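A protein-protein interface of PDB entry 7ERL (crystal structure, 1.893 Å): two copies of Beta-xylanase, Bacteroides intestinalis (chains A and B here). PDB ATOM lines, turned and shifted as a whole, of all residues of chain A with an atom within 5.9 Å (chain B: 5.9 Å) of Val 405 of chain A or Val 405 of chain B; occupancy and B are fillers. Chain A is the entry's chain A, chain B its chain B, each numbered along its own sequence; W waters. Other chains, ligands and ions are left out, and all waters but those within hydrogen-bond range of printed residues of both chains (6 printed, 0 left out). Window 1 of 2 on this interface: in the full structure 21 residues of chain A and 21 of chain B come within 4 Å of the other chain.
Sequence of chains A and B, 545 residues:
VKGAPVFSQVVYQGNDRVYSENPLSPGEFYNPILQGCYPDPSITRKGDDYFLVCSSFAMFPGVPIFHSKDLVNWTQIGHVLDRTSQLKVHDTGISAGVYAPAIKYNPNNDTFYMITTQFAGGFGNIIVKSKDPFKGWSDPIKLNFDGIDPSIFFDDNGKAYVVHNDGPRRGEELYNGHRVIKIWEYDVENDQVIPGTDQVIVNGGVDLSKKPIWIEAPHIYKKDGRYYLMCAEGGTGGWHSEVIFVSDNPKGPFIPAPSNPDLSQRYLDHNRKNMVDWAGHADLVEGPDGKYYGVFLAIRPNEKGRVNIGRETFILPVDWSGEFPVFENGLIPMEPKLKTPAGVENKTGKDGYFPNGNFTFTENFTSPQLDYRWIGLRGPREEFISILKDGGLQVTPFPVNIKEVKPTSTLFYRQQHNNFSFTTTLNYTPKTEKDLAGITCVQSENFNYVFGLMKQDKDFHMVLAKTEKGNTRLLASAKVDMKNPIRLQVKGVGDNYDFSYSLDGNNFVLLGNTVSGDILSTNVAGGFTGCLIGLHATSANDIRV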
ATOM      1  N   HIS A  90       7.831 -11.582  33.638  1.00  0.00           N
ATOM      2  CA  HIS A  90       7.463 -10.932  32.378  1.00  0.00           C
ATOM      3  C   HIS A  90       8.670 -10.429  31.587  1.00  0.00           C
ATOM      4  O   HIS A  90       8.785 -10.670  30.378  1.00  0.00           O
ATOM      5  CB  HIS A  90       6.507  -9.776  32.708  1.00  0.00           C
ATOM      6  CG  HIS A  90       5.728  -9.257  31.545  1.00  0.00           C
ATOM      7  ND1 HIS A  90       6.242  -8.338  30.654  1.00  0.00           N
ATOM      8  CD2 HIS A  90       4.452  -9.489  31.149  1.00  0.00           C
ATOM      9  CE1 HIS A  90       5.325  -8.042  29.750  1.00  0.00           C
ATOM     10  NE2 HIS A  90       4.229  -8.725  30.029  1.00  0.00           N
ATOM     11  N   ASP A  91       9.592  -9.743  32.269  1.00  0.00           N
ATOM     12  CA  ASP A  91      10.724  -9.079  31.634  1.00  0.00           C
ATOM     13  C   ASP A  91      12.058  -9.699  32.042  1.00  0.00           C
ATOM     14  O   ASP A  91      13.087  -9.024  32.010  1.00  0.00           O
ATOM     15  CB  ASP A  91      10.732  -7.584  31.993  1.00  0.00           C
ATOM     16  CG  ASP A  91       9.507  -6.849  31.485  1.00  0.00           C
ATOM     17  OD1 ASP A  91       9.119  -7.059  30.320  1.00  0.00           O
ATOM     18  OD2 ASP A  91       8.930  -6.050  32.250  1.00  0.00           O
ATOM     19  N   THR A  92      12.071 -10.955  32.456  1.00  0.00           N
ATOM     20  CA  THR A  92      13.211 -11.479  33.199  1.00  0.00           C
ATOM     21  C   THR A  92      14.213 -12.177  32.281  1.00  0.00           C
ATOM     22  O   THR A  92      13.827 -12.896  31.351  1.00  0.00           O
ATOM     23  CB  THR A  92      12.710 -12.442  34.288  1.00  0.00           C
ATOM     24  OG1 THR A  92      11.964 -11.688  35.258  1.00  0.00           O
ATOM     25  CG2 THR A  92      13.853 -13.136  34.984  1.00  0.00           C
ATOM     26  N   GLY A  93      15.505 -11.983  32.567  1.00  0.00           N
ATOM     27  CA  GLY A  93      16.534 -12.661  31.794  1.00  0.00           C
ATOM     28  C   GLY A  93      16.436 -14.171  31.915  1.00  0.00           C
ATOM     29  O   GLY A  93      15.960 -14.706  32.911  1.00  0.00           O
ATOM     30  N   ARG A 378       8.303 -16.758  30.426  1.00  0.00           N
ATOM     31  CA  ARG A 378       8.083 -15.389  30.894  1.00  0.00           C
ATOM     32  C   ARG A 378       6.619 -15.048  31.183  1.00  0.00           C
ATOM     33  O   ARG A 378       6.350 -14.086  31.899  1.00  0.00           O
ATOM     34  CB  ARG A 378       8.669 -14.370  29.902  1.00  0.00           C
ATOM     35  CG  ARG A 378      10.209 -14.376  29.912  1.00  0.00           C
ATOM     36  CD  ARG A 378      10.876 -13.315  29.010  1.00  0.00           C
ATOM     37  NE  ARG A 378      12.327 -13.405  29.223  1.00  0.00           N
ATOM     38  CZ  ARG A 378      13.201 -13.931  28.370  1.00  0.00           C
ATOM     39  NH1 ARG A 378      12.813 -14.388  27.185  1.00  0.00           N
ATOM     40  NH2 ARG A 378      14.488 -13.988  28.701  1.00  0.00           N
ATOM     41  N   ASN A 401       8.225 -10.873  18.834  1.00  0.00           N
ATOM     42  CA  ASN A 401       9.234 -11.692  18.174  1.00  0.00           C
ATOM     43  C   ASN A 401       9.932 -12.601  19.189  1.00  0.00           C
ATOM     44  O   ASN A 401      10.033 -12.273  20.383  1.00  0.00           O
ATOM     45  CB  ASN A 401      10.245 -10.770  17.483  1.00  0.00           C
ATOM     46  CG  ASN A 401      11.191 -11.501  16.557  1.00  0.00           C
ATOM     47  OD1 ASN A 401      12.246 -11.990  16.981  1.00  0.00           O
ATOM     48  ND2 ASN A 401      10.845 -11.542  15.268  1.00  0.00           N
ATOM     49  N   LYS A 403      12.900 -12.985  19.672  1.00  0.00           N
ATOM     50  CA  LYS A 403      14.095 -12.336  20.207  1.00  0.00           C
ATOM     51  C   LYS A 403      13.808 -11.408  21.385  1.00  0.00           C
ATOM     52  O   LYS A 403      14.753 -10.978  22.059  1.00  0.00           O
ATOM     53  CB  LYS A 403      14.798 -11.530  19.102  1.00  0.00           C
ATOM     54  CG  LYS A 403      15.559 -12.376  18.061  1.00  0.00           C
ATOM     55  CD  LYS A 403      16.304 -11.482  17.053  1.00  0.00           C
ATOM     56  CE  LYS A 403      15.335 -10.844  16.050  1.00  0.00           C
ATOM     57  NZ  LYS A 403      14.565 -11.888  15.312  1.00  0.00           N
ATOM     58  N   GLU A 404      12.549 -11.096  21.656  1.00  0.00           N
ATOM     59  CA  GLU A 404      12.220 -10.109  22.675  1.00  0.00           C
ATOM     60  C   GLU A 404      12.269 -10.717  24.069  1.00  0.00           C
ATOM     61  O   GLU A 404      11.917 -11.883  24.278  1.00  0.00           O
ATOM     62  CB  GLU A 404      10.829  -9.524  22.423  1.00  0.00           C
ATOM     63  CG  GLU A 404      10.750  -8.734  21.123  1.00  0.00           C
ATOM     64  CD  GLU A 404       9.387  -8.123  20.891  1.00  0.00           C
ATOM     65  OE1 GLU A 404       8.882  -7.424  21.790  1.00  0.00           O
ATOM     66  OE2 GLU A 404       8.819  -8.339  19.801  1.00  0.00           O
ATOM     67  N   VAL A 405      12.699  -9.906  25.035  1.00  0.00           N
ATOM     68  CA  VAL A 405      12.677 -10.325  26.429  1.00  0.00           C
ATOM     69  C   VAL A 405      11.291  -9.980  26.960  1.00  0.00           C
ATOM     70  O   VAL A 405      11.118  -9.058  27.769  1.00  0.00           O
ATOM     71  CB  VAL A 405      13.829  -9.676  27.218  1.00  0.00           C
ATOM     72  CG1 VAL A 405      13.903 -10.222  28.639  1.00  0.00           C
ATOM     73  CG2 VAL A 405      15.159  -9.960  26.499  1.00  0.00           C
ATOM     74  N   LYS A 406      10.293 -10.714  26.470  1.00  0.00           N
ATOM     75  CA  LYS A 406       8.872 -10.496  26.711  1.00  0.00           C
ATOM     76  C   LYS A 406       8.169 -11.836  26.567  1.00  0.00           C
ATOM     77  O   LYS A 406       8.680 -12.734  25.885  1.00  0.00           O
ATOM     78  CB  LYS A 406       8.271  -9.499  25.701  1.00  0.00           C
ATOM     79  CG  LYS A 406       8.793  -8.073  25.767  1.00  0.00           C
ATOM     80  CD  LYS A 406       8.256  -7.375  27.018  1.00  0.00           C
ATOM     81  CE  LYS A 406       8.687  -5.911  27.073  1.00  0.00           C
ATOM     82  NZ  LYS A 406       8.254  -5.314  28.382  1.00  0.00           N
ATOM     83  N   PRO A 407       6.984 -11.996  27.159  1.00  0.00           N
ATOM     84  CA  PRO A 407       6.210 -13.228  26.908  1.00  0.00           C
ATOM     85  C   PRO A 407       5.824 -13.345  25.443  1.00  0.00           C
ATOM     86  O   PRO A 407       5.181 -12.454  24.884  1.00  0.00           O
ATOM     87  CB  PRO A 407       4.969 -13.055  27.793  1.00  0.00           C
ATOM     88  CG  PRO A 407       5.405 -12.067  28.886  1.00  0.00           C
ATOM     89  CD  PRO A 407       6.321 -11.118  28.143  1.00  0.00           C
ATOM     90  N   GLU A 445      15.946 -16.230  24.129  1.00  0.00           N
ATOM     91  CA  GLU A 445      15.626 -15.320  23.038  1.00  0.00           C
ATOM     92  C   GLU A 445      16.844 -15.021  22.162  1.00  0.00           C
ATOM     93  O   GLU A 445      16.669 -14.623  21.012  1.00  0.00           O
ATOM     94  CB  GLU A 445      15.035 -14.024  23.613  1.00  0.00           C
ATOM     95  CG  GLU A 445      16.035 -13.115  24.361  1.00  0.00           C
ATOM     96  CD  GLU A 445      16.338 -13.552  25.789  1.00  0.00           C
ATOM     97  OE1 GLU A 445      15.813 -14.600  26.252  1.00  0.00           O
ATOM     98  OE2 GLU A 445      17.123 -12.846  26.454  1.00  0.00           O
ATOM     99  N   ASN A 446      18.067 -15.228  22.664  1.00  0.00           N
ATOM    100  CA  ASN A 446      19.285 -14.933  21.913  1.00  0.00           C
ATOM    101  C   ASN A 446      19.878 -16.148  21.214  1.00  0.00           C
ATOM    102  O   ASN A 446      20.768 -15.985  20.358  1.00  0.00           O
ATOM    103  CB  ASN A 446      20.337 -14.324  22.845  1.00  0.00           C
ATOM    104  CG  ASN A 446      19.944 -12.944  23.339  1.00  0.00           C
ATOM    105  OD1 ASN A 446      19.591 -12.071  22.547  1.00  0.00           O
ATOM    106  ND2 ASN A 446      19.983 -12.746  24.652  1.00  0.00           N
ATOM    107  N   HIS B  90      16.930  -2.124  19.049  1.00  0.00           N
ATOM    108  CA  HIS B  90      15.704  -1.920  19.837  1.00  0.00           C
ATOM    109  C   HIS B  90      15.539  -2.965  20.942  1.00  0.00           C
ATOM    110  O   HIS B  90      15.208  -2.623  22.091  1.00  0.00           O
ATOM    111  CB  HIS B  90      14.497  -1.935  18.879  1.00  0.00           C
ATOM    112  CG  HIS B  90      13.204  -1.452  19.475  1.00  0.00           C
ATOM    113  ND1 HIS B  90      12.379  -2.261  20.227  1.00  0.00           N
ATOM    114  CD2 HIS B  90      12.559  -0.263  19.367  1.00  0.00           C
ATOM    115  CE1 HIS B  90      11.301  -1.584  20.587  1.00  0.00           C
ATOM    116  NE2 HIS B  90      11.387  -0.366  20.080  1.00  0.00           N
ATOM    117  N   ASP B  91      15.768  -4.246  20.619  1.00  0.00           N
ATOM    118  CA  ASP B  91      15.573  -5.346  21.562  1.00  0.00           C
ATOM    119  C   ASP B  91      16.882  -6.051  21.924  1.00  0.00           C
ATOM    120  O   ASP B  91      16.866  -7.225  22.304  1.00  0.00           O
ATOM    121  CB  ASP B  91      14.595  -6.373  20.987  1.00  0.00           C
ATOM    122  CG  ASP B  91      13.257  -5.768  20.613  1.00  0.00           C
ATOM    123  OD1 ASP B  91      12.648  -5.079  21.458  1.00  0.00           O
ATOM    124  OD2 ASP B  91      12.811  -5.990  19.466  1.00  0.00           O
ATOM    125  N   THR B  92      18.011  -5.373  21.802  1.00  0.00           N
ATOM    126  CA  THR B  92      19.309  -6.039  21.822  1.00  0.00           C
ATOM    127  C   THR B  92      19.887  -6.110  23.238  1.00  0.00           C
ATOM    128  O   THR B  92      19.786  -5.151  24.016  1.00  0.00           O
ATOM    129  CB  THR B  92      20.255  -5.293  20.873  1.00  0.00           C
ATOM    130  OG1 THR B  92      19.798  -5.491  19.531  1.00  0.00           O
ATOM    131  CG2 THR B  92      21.684  -5.771  20.987  1.00  0.00           C
ATOM    132  N   GLY B  93      20.486  -7.257  23.570  1.00  0.00           N
ATOM    133  CA  GLY B  93      21.122  -7.401  24.870  1.00  0.00           C
ATOM    134  C   GLY B  93      22.275  -6.429  25.041  1.00  0.00           C
ATOM    135  O   GLY B  93      22.883  -5.982  24.073  1.00  0.00           O
ATOM    136  N   ARG B 378      19.558   1.627  23.188  1.00  0.00           N
ATOM    137  CA  ARG B 378      18.653   0.805  22.378  1.00  0.00           C
ATOM    138  C   ARG B 378      17.779   1.602  21.409  1.00  0.00           C
ATOM    139  O   ARG B 378      17.295   1.039  20.422  1.00  0.00           O
ATOM    140  CB  ARG B 378      17.763  -0.078  23.263  1.00  0.00           C
ATOM    141  CG  ARG B 378      18.556  -1.169  23.995  1.00  0.00           C
ATOM    142  CD  ARG B 378      17.666  -2.093  24.825  1.00  0.00           C
ATOM    143  NE  ARG B 378      18.484  -3.199  25.301  1.00  0.00           N
ATOM    144  CZ  ARG B 378      18.908  -3.330  26.550  1.00  0.00           C
ATOM    145  NH1 ARG B 378      18.549  -2.440  27.478  1.00  0.00           N
ATOM    146  NH2 ARG B 378      19.694  -4.351  26.874  1.00  0.00           N
ATOM    147  N   ASN B 401       9.887   0.482  31.849  1.00  0.00           N
ATOM    148  CA  ASN B 401      10.674   0.423  33.068  1.00  0.00           C
ATOM    149  C   ASN B 401      12.154   0.265  32.714  1.00  0.00           C
ATOM    150  O   ASN B 401      12.507  -0.333  31.689  1.00  0.00           O
ATOM    151  CB  ASN B 401      10.170  -0.755  33.916  1.00  0.00           C
ATOM    152  CG  ASN B 401      10.700  -0.745  35.323  1.00  0.00           C
ATOM    153  OD1 ASN B 401      11.769  -1.304  35.599  1.00  0.00           O
ATOM    154  ND2 ASN B 401       9.944  -0.130  36.245  1.00  0.00           N
ATOM    155  N   LYS B 403      14.094  -1.744  33.738  1.00  0.00           N
ATOM    156  CA  LYS B 403      14.439  -3.163  33.701  1.00  0.00           C
ATOM    157  C   LYS B 403      14.155  -3.832  32.357  1.00  0.00           C
ATOM    158  O   LYS B 403      14.604  -4.969  32.141  1.00  0.00           O
ATOM    159  CB  LYS B 403      13.684  -3.918  34.799  1.00  0.00           C
ATOM    160  CG  LYS B 403      14.339  -3.824  36.164  1.00  0.00           C
ATOM    161  CD  LYS B 403      13.609  -4.714  37.178  1.00  0.00           C
ATOM    162  CE  LYS B 403      12.198  -4.208  37.415  1.00  0.00           C
ATOM    163  NZ  LYS B 403      12.217  -2.793  37.923  1.00  0.00           N
ATOM    164  N   GLU B 404      13.444  -3.170  31.453  1.00  0.00           N
ATOM    165  CA  GLU B 404      13.056  -3.794  30.193  1.00  0.00           C
ATOM    166  C   GLU B 404      14.178  -3.750  29.157  1.00  0.00           C
ATOM    167  O   GLU B 404      14.974  -2.806  29.105  1.00  0.00           O
ATOM    168  CB  GLU B 404      11.809  -3.114  29.633  1.00  0.00           C
ATOM    169  CG  GLU B 404      10.618  -3.185  30.582  1.00  0.00           C
ATOM    170  CD  GLU B 404       9.375  -2.537  30.009  1.00  0.00           C
ATOM    171  OE1 GLU B 404       9.053  -2.809  28.829  1.00  0.00           O
ATOM    172  OE2 GLU B 404       8.728  -1.740  30.735  1.00  0.00           O
ATOM    173  N   VAL B 405      14.233  -4.791  28.316  1.00  0.00           N
ATOM    174  CA  VAL B 405      15.151  -4.801  27.181  1.00  0.00           C
ATOM    175  C   VAL B 405      14.415  -4.118  26.039  1.00  0.00           C
ATOM    176  O   VAL B 405      13.993  -4.757  25.063  1.00  0.00           O
ATOM    177  CB  VAL B 405      15.621  -6.228  26.824  1.00  0.00           C
ATOM    178  CG1 VAL B 405      16.650  -6.226  25.646  1.00  0.00           C
ATOM    179  CG2 VAL B 405      16.232  -6.876  28.056  1.00  0.00           C
ATOM    180  N   LYS B 406      14.237  -2.810  26.184  1.00  0.00           N
ATOM    181  CA  LYS B 406      13.475  -1.962  25.284  1.00  0.00           C
ATOM    182  C   LYS B 406      14.044  -0.559  25.394  1.00  0.00           C
ATOM    183  O   LYS B 406      14.679  -0.226  26.400  1.00  0.00           O
ATOM    184  CB  LYS B 406      11.981  -1.936  25.654  1.00  0.00           C
ATOM    185  CG  LYS B 406      11.246  -3.254  25.499  1.00  0.00           C
ATOM    186  CD  LYS B 406      11.152  -3.638  24.025  1.00  0.00           C
ATOM    187  CE  LYS B 406      10.317  -4.899  23.822  1.00  0.00           C
ATOM    188  NZ  LYS B 406      10.191  -5.167  22.357  1.00  0.00           N
ATOM    189  N   PRO B 407      13.830   0.287  24.395  1.00  0.00           N
ATOM    190  CA  PRO B 407      14.230   1.692  24.546  1.00  0.00           C
ATOM    191  C   PRO B 407      13.455   2.359  25.673  1.00  0.00           C
ATOM    192  O   PRO B 407      12.220   2.304  25.725  1.00  0.00           O
ATOM    193  CB  PRO B 407      13.893   2.308  23.183  1.00  0.00           C
ATOM    194  CG  PRO B 407      13.922   1.117  22.219  1.00  0.00           C
ATOM    195  CD  PRO B 407      13.333  -0.001  23.034  1.00  0.00           C
ATOM    196  N   GLU B 445      20.055  -3.055  32.023  1.00  0.00           N
ATOM    197  CA  GLU B 445      18.721  -3.121  32.600  1.00  0.00           C
ATOM    198  C   GLU B 445      18.687  -3.990  33.854  1.00  0.00           C
ATOM    199  O   GLU B 445      17.764  -3.851  34.664  1.00  0.00           O
ATOM    200  CB  GLU B 445      17.737  -3.648  31.550  1.00  0.00           C
ATOM    201  CG  GLU B 445      17.939  -5.130  31.203  1.00  0.00           C
ATOM    202  CD  GLU B 445      19.037  -5.382  30.177  1.00  0.00           C
ATOM    203  OE1 GLU B 445      19.724  -4.423  29.739  1.00  0.00           O
ATOM    204  OE2 GLU B 445      19.218  -6.558  29.803  1.00  0.00           O
ATOM    205  N   ASN B 446      19.675  -4.877  34.037  1.00  0.00           N
ATOM    206  CA  ASN B 446      19.721  -5.799  35.173  1.00  0.00           C
ATOM    207  C   ASN B 446      20.630  -5.332  36.300  1.00  0.00           C
ATOM    208  O   ASN B 446      20.597  -5.930  37.381  1.00  0.00           O
ATOM    209  CB  ASN B 446      20.174  -7.191  34.704  1.00  0.00           C
ATOM    210  CG  ASN B 446      19.153  -7.856  33.800  1.00  0.00           C
ATOM    211  OD1 ASN B 446      17.980  -7.942  34.145  1.00  0.00           O
ATOM    212  ND2 ASN B 446      19.592  -8.316  32.637  1.00  0.00           N
HETATM  213  O   HOH W   1      16.729 -10.279  34.477  1.00  0.00           O
HETATM  214  O   HOH W   2      13.464  -7.395  24.208  1.00  0.00           O
HETATM  215  O   HOH W   3      20.830  -9.612  22.093  1.00  0.00           O
HETATM  216  O   HOH W   4      12.260  -6.837  28.898  1.00  0.00           O
HETATM  217  O   HOH W   5      15.232  -7.779  31.332  1.00  0.00           O
HETATM  218  O   HOH W   6      16.667  -9.389  23.380  1.00  0.00           O
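Water W6 bridges O of Asp 91 of chain B and O of Lys 403 of chain A. Water W5 lies within hydrogen-bond range of O of Asp 91 of chain A and O of Lys 403 of chain B. Water W1 bridges OD1 of Asn 446 of chain B (2.7 Å) and N of Gly 93 of chain A (2.8 Å). Water W4 lies within hydrogen-bond range of O of Val 405 of chain A (2.7 Å), N of Val 405 of chain B (2.9 Å) and OD1 of Asp 91 of chain A (3.5 Å). Water W2 bridges N of Val 405 of chain A (2.8 Å) and O of Val 405 of chain B (2.8 Å). Water W3 bridges the side-chain amide oxygen (OD1) of Asn 446 of chain A (2.8 Å) and the backbone NH (N) of Gly 93 of chain B (2.8 Å).
OD2 of Asp 91 of chain A touches CG of Glu 404 of chain B, 3.7 Å away. CG of Glu 404 of chain A touches OD2 of Asp 91 of chain B (3.8 Å). Val 405 of chain A touches Val 405 of chain B. Lys 406 of chain B touches Lys 406 of chain A (CE to CE, 3.8 Å).
NZ of Lys 406 of chain B is in salt-bridge range of OE1 of Glu 404 of chain A (2.7 Å). The side-chain amino group (NZ) of Lys 406 of chain A lies within salt-bridge range of the side-chain carboxylate (OE1) of Glu 404 of chain B (2.7 Å).
Of the printed residues of chain B, Glu 404 of chain A touches Asp 91 and Lys 406. Val 405 of chain A touches just one residue of chain B: Val 405 (3.6 Å). Of the printed residues of chain A, Asp 91 of chain B touches Glu 404 (3.8 Å). Of chain A, only Val 405 comes within 4 Å of Val 405 of chain B. The nearest residue of chain B that does not touch Val 405 of chain A is Asp 91 of chain B (5.3 Å).
A ring nitrogen (ND1) of His 90 of chain A sits at hydrogen-bond distance from the side-chain carboxylate of Asp 91 of chain A, 3.2 Å away. The side-chain carboxylate (OD1) of Asp 91 of chain A lies within salt-bridge range of the side-chain amino group (NZ) of Lys 406 of chain A. OE2 of Glu 404 of chain A is in hydrogen-bond range of N of Asn 401 of chain A (2.8 Å). OD1 of Asp 91 of chain B sits at hydrogen-bond distance from ND1 of His 90 of chain B (3.1 Å). OD1 of Asp 91 of chain B is in salt-bridge range of NZ of Lys 406 of chain B (2.6 Å). The side-chain carboxylate (OE2) of Glu 404 of chain B is in hydrogen-bond range of the backbone NH (N) of Asn 401 of chain B, 2.7 Å away.
Asp 91 of chain A touches Glu 404 of chain B, and with the chains exchanged Glu 404 of chain A touches Asp 91 of chain B. Glu 404 of chain A touches Lys 406 of chain B, and with the chains exchanged Lys 406 of chain A touches Glu 404 of chain B. Val 405 of chain B touches its own counterpart, Val 405 of chain A. Lys 406 of chain A touches its own counterpart, Lys 406 of chain B.
Of the 13 printed residues of chain A, 4 touch a printed residue of chain B. Hydrophobic or aromatic side chains of chain A that line the printed part of chain B: Val 405. Of the 13 printed residues of chain B, 4 touch a printed residue of chain A. Printed residues of chain B that touch a printed residue of chain A: Asp 91, Glu 404, Val 405 and Lys 406. Hydrophobic or aromatic side chains of chain B that line the printed part of chain A: Val 405. Among the printed residues, 6 pairs touch across the chains.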
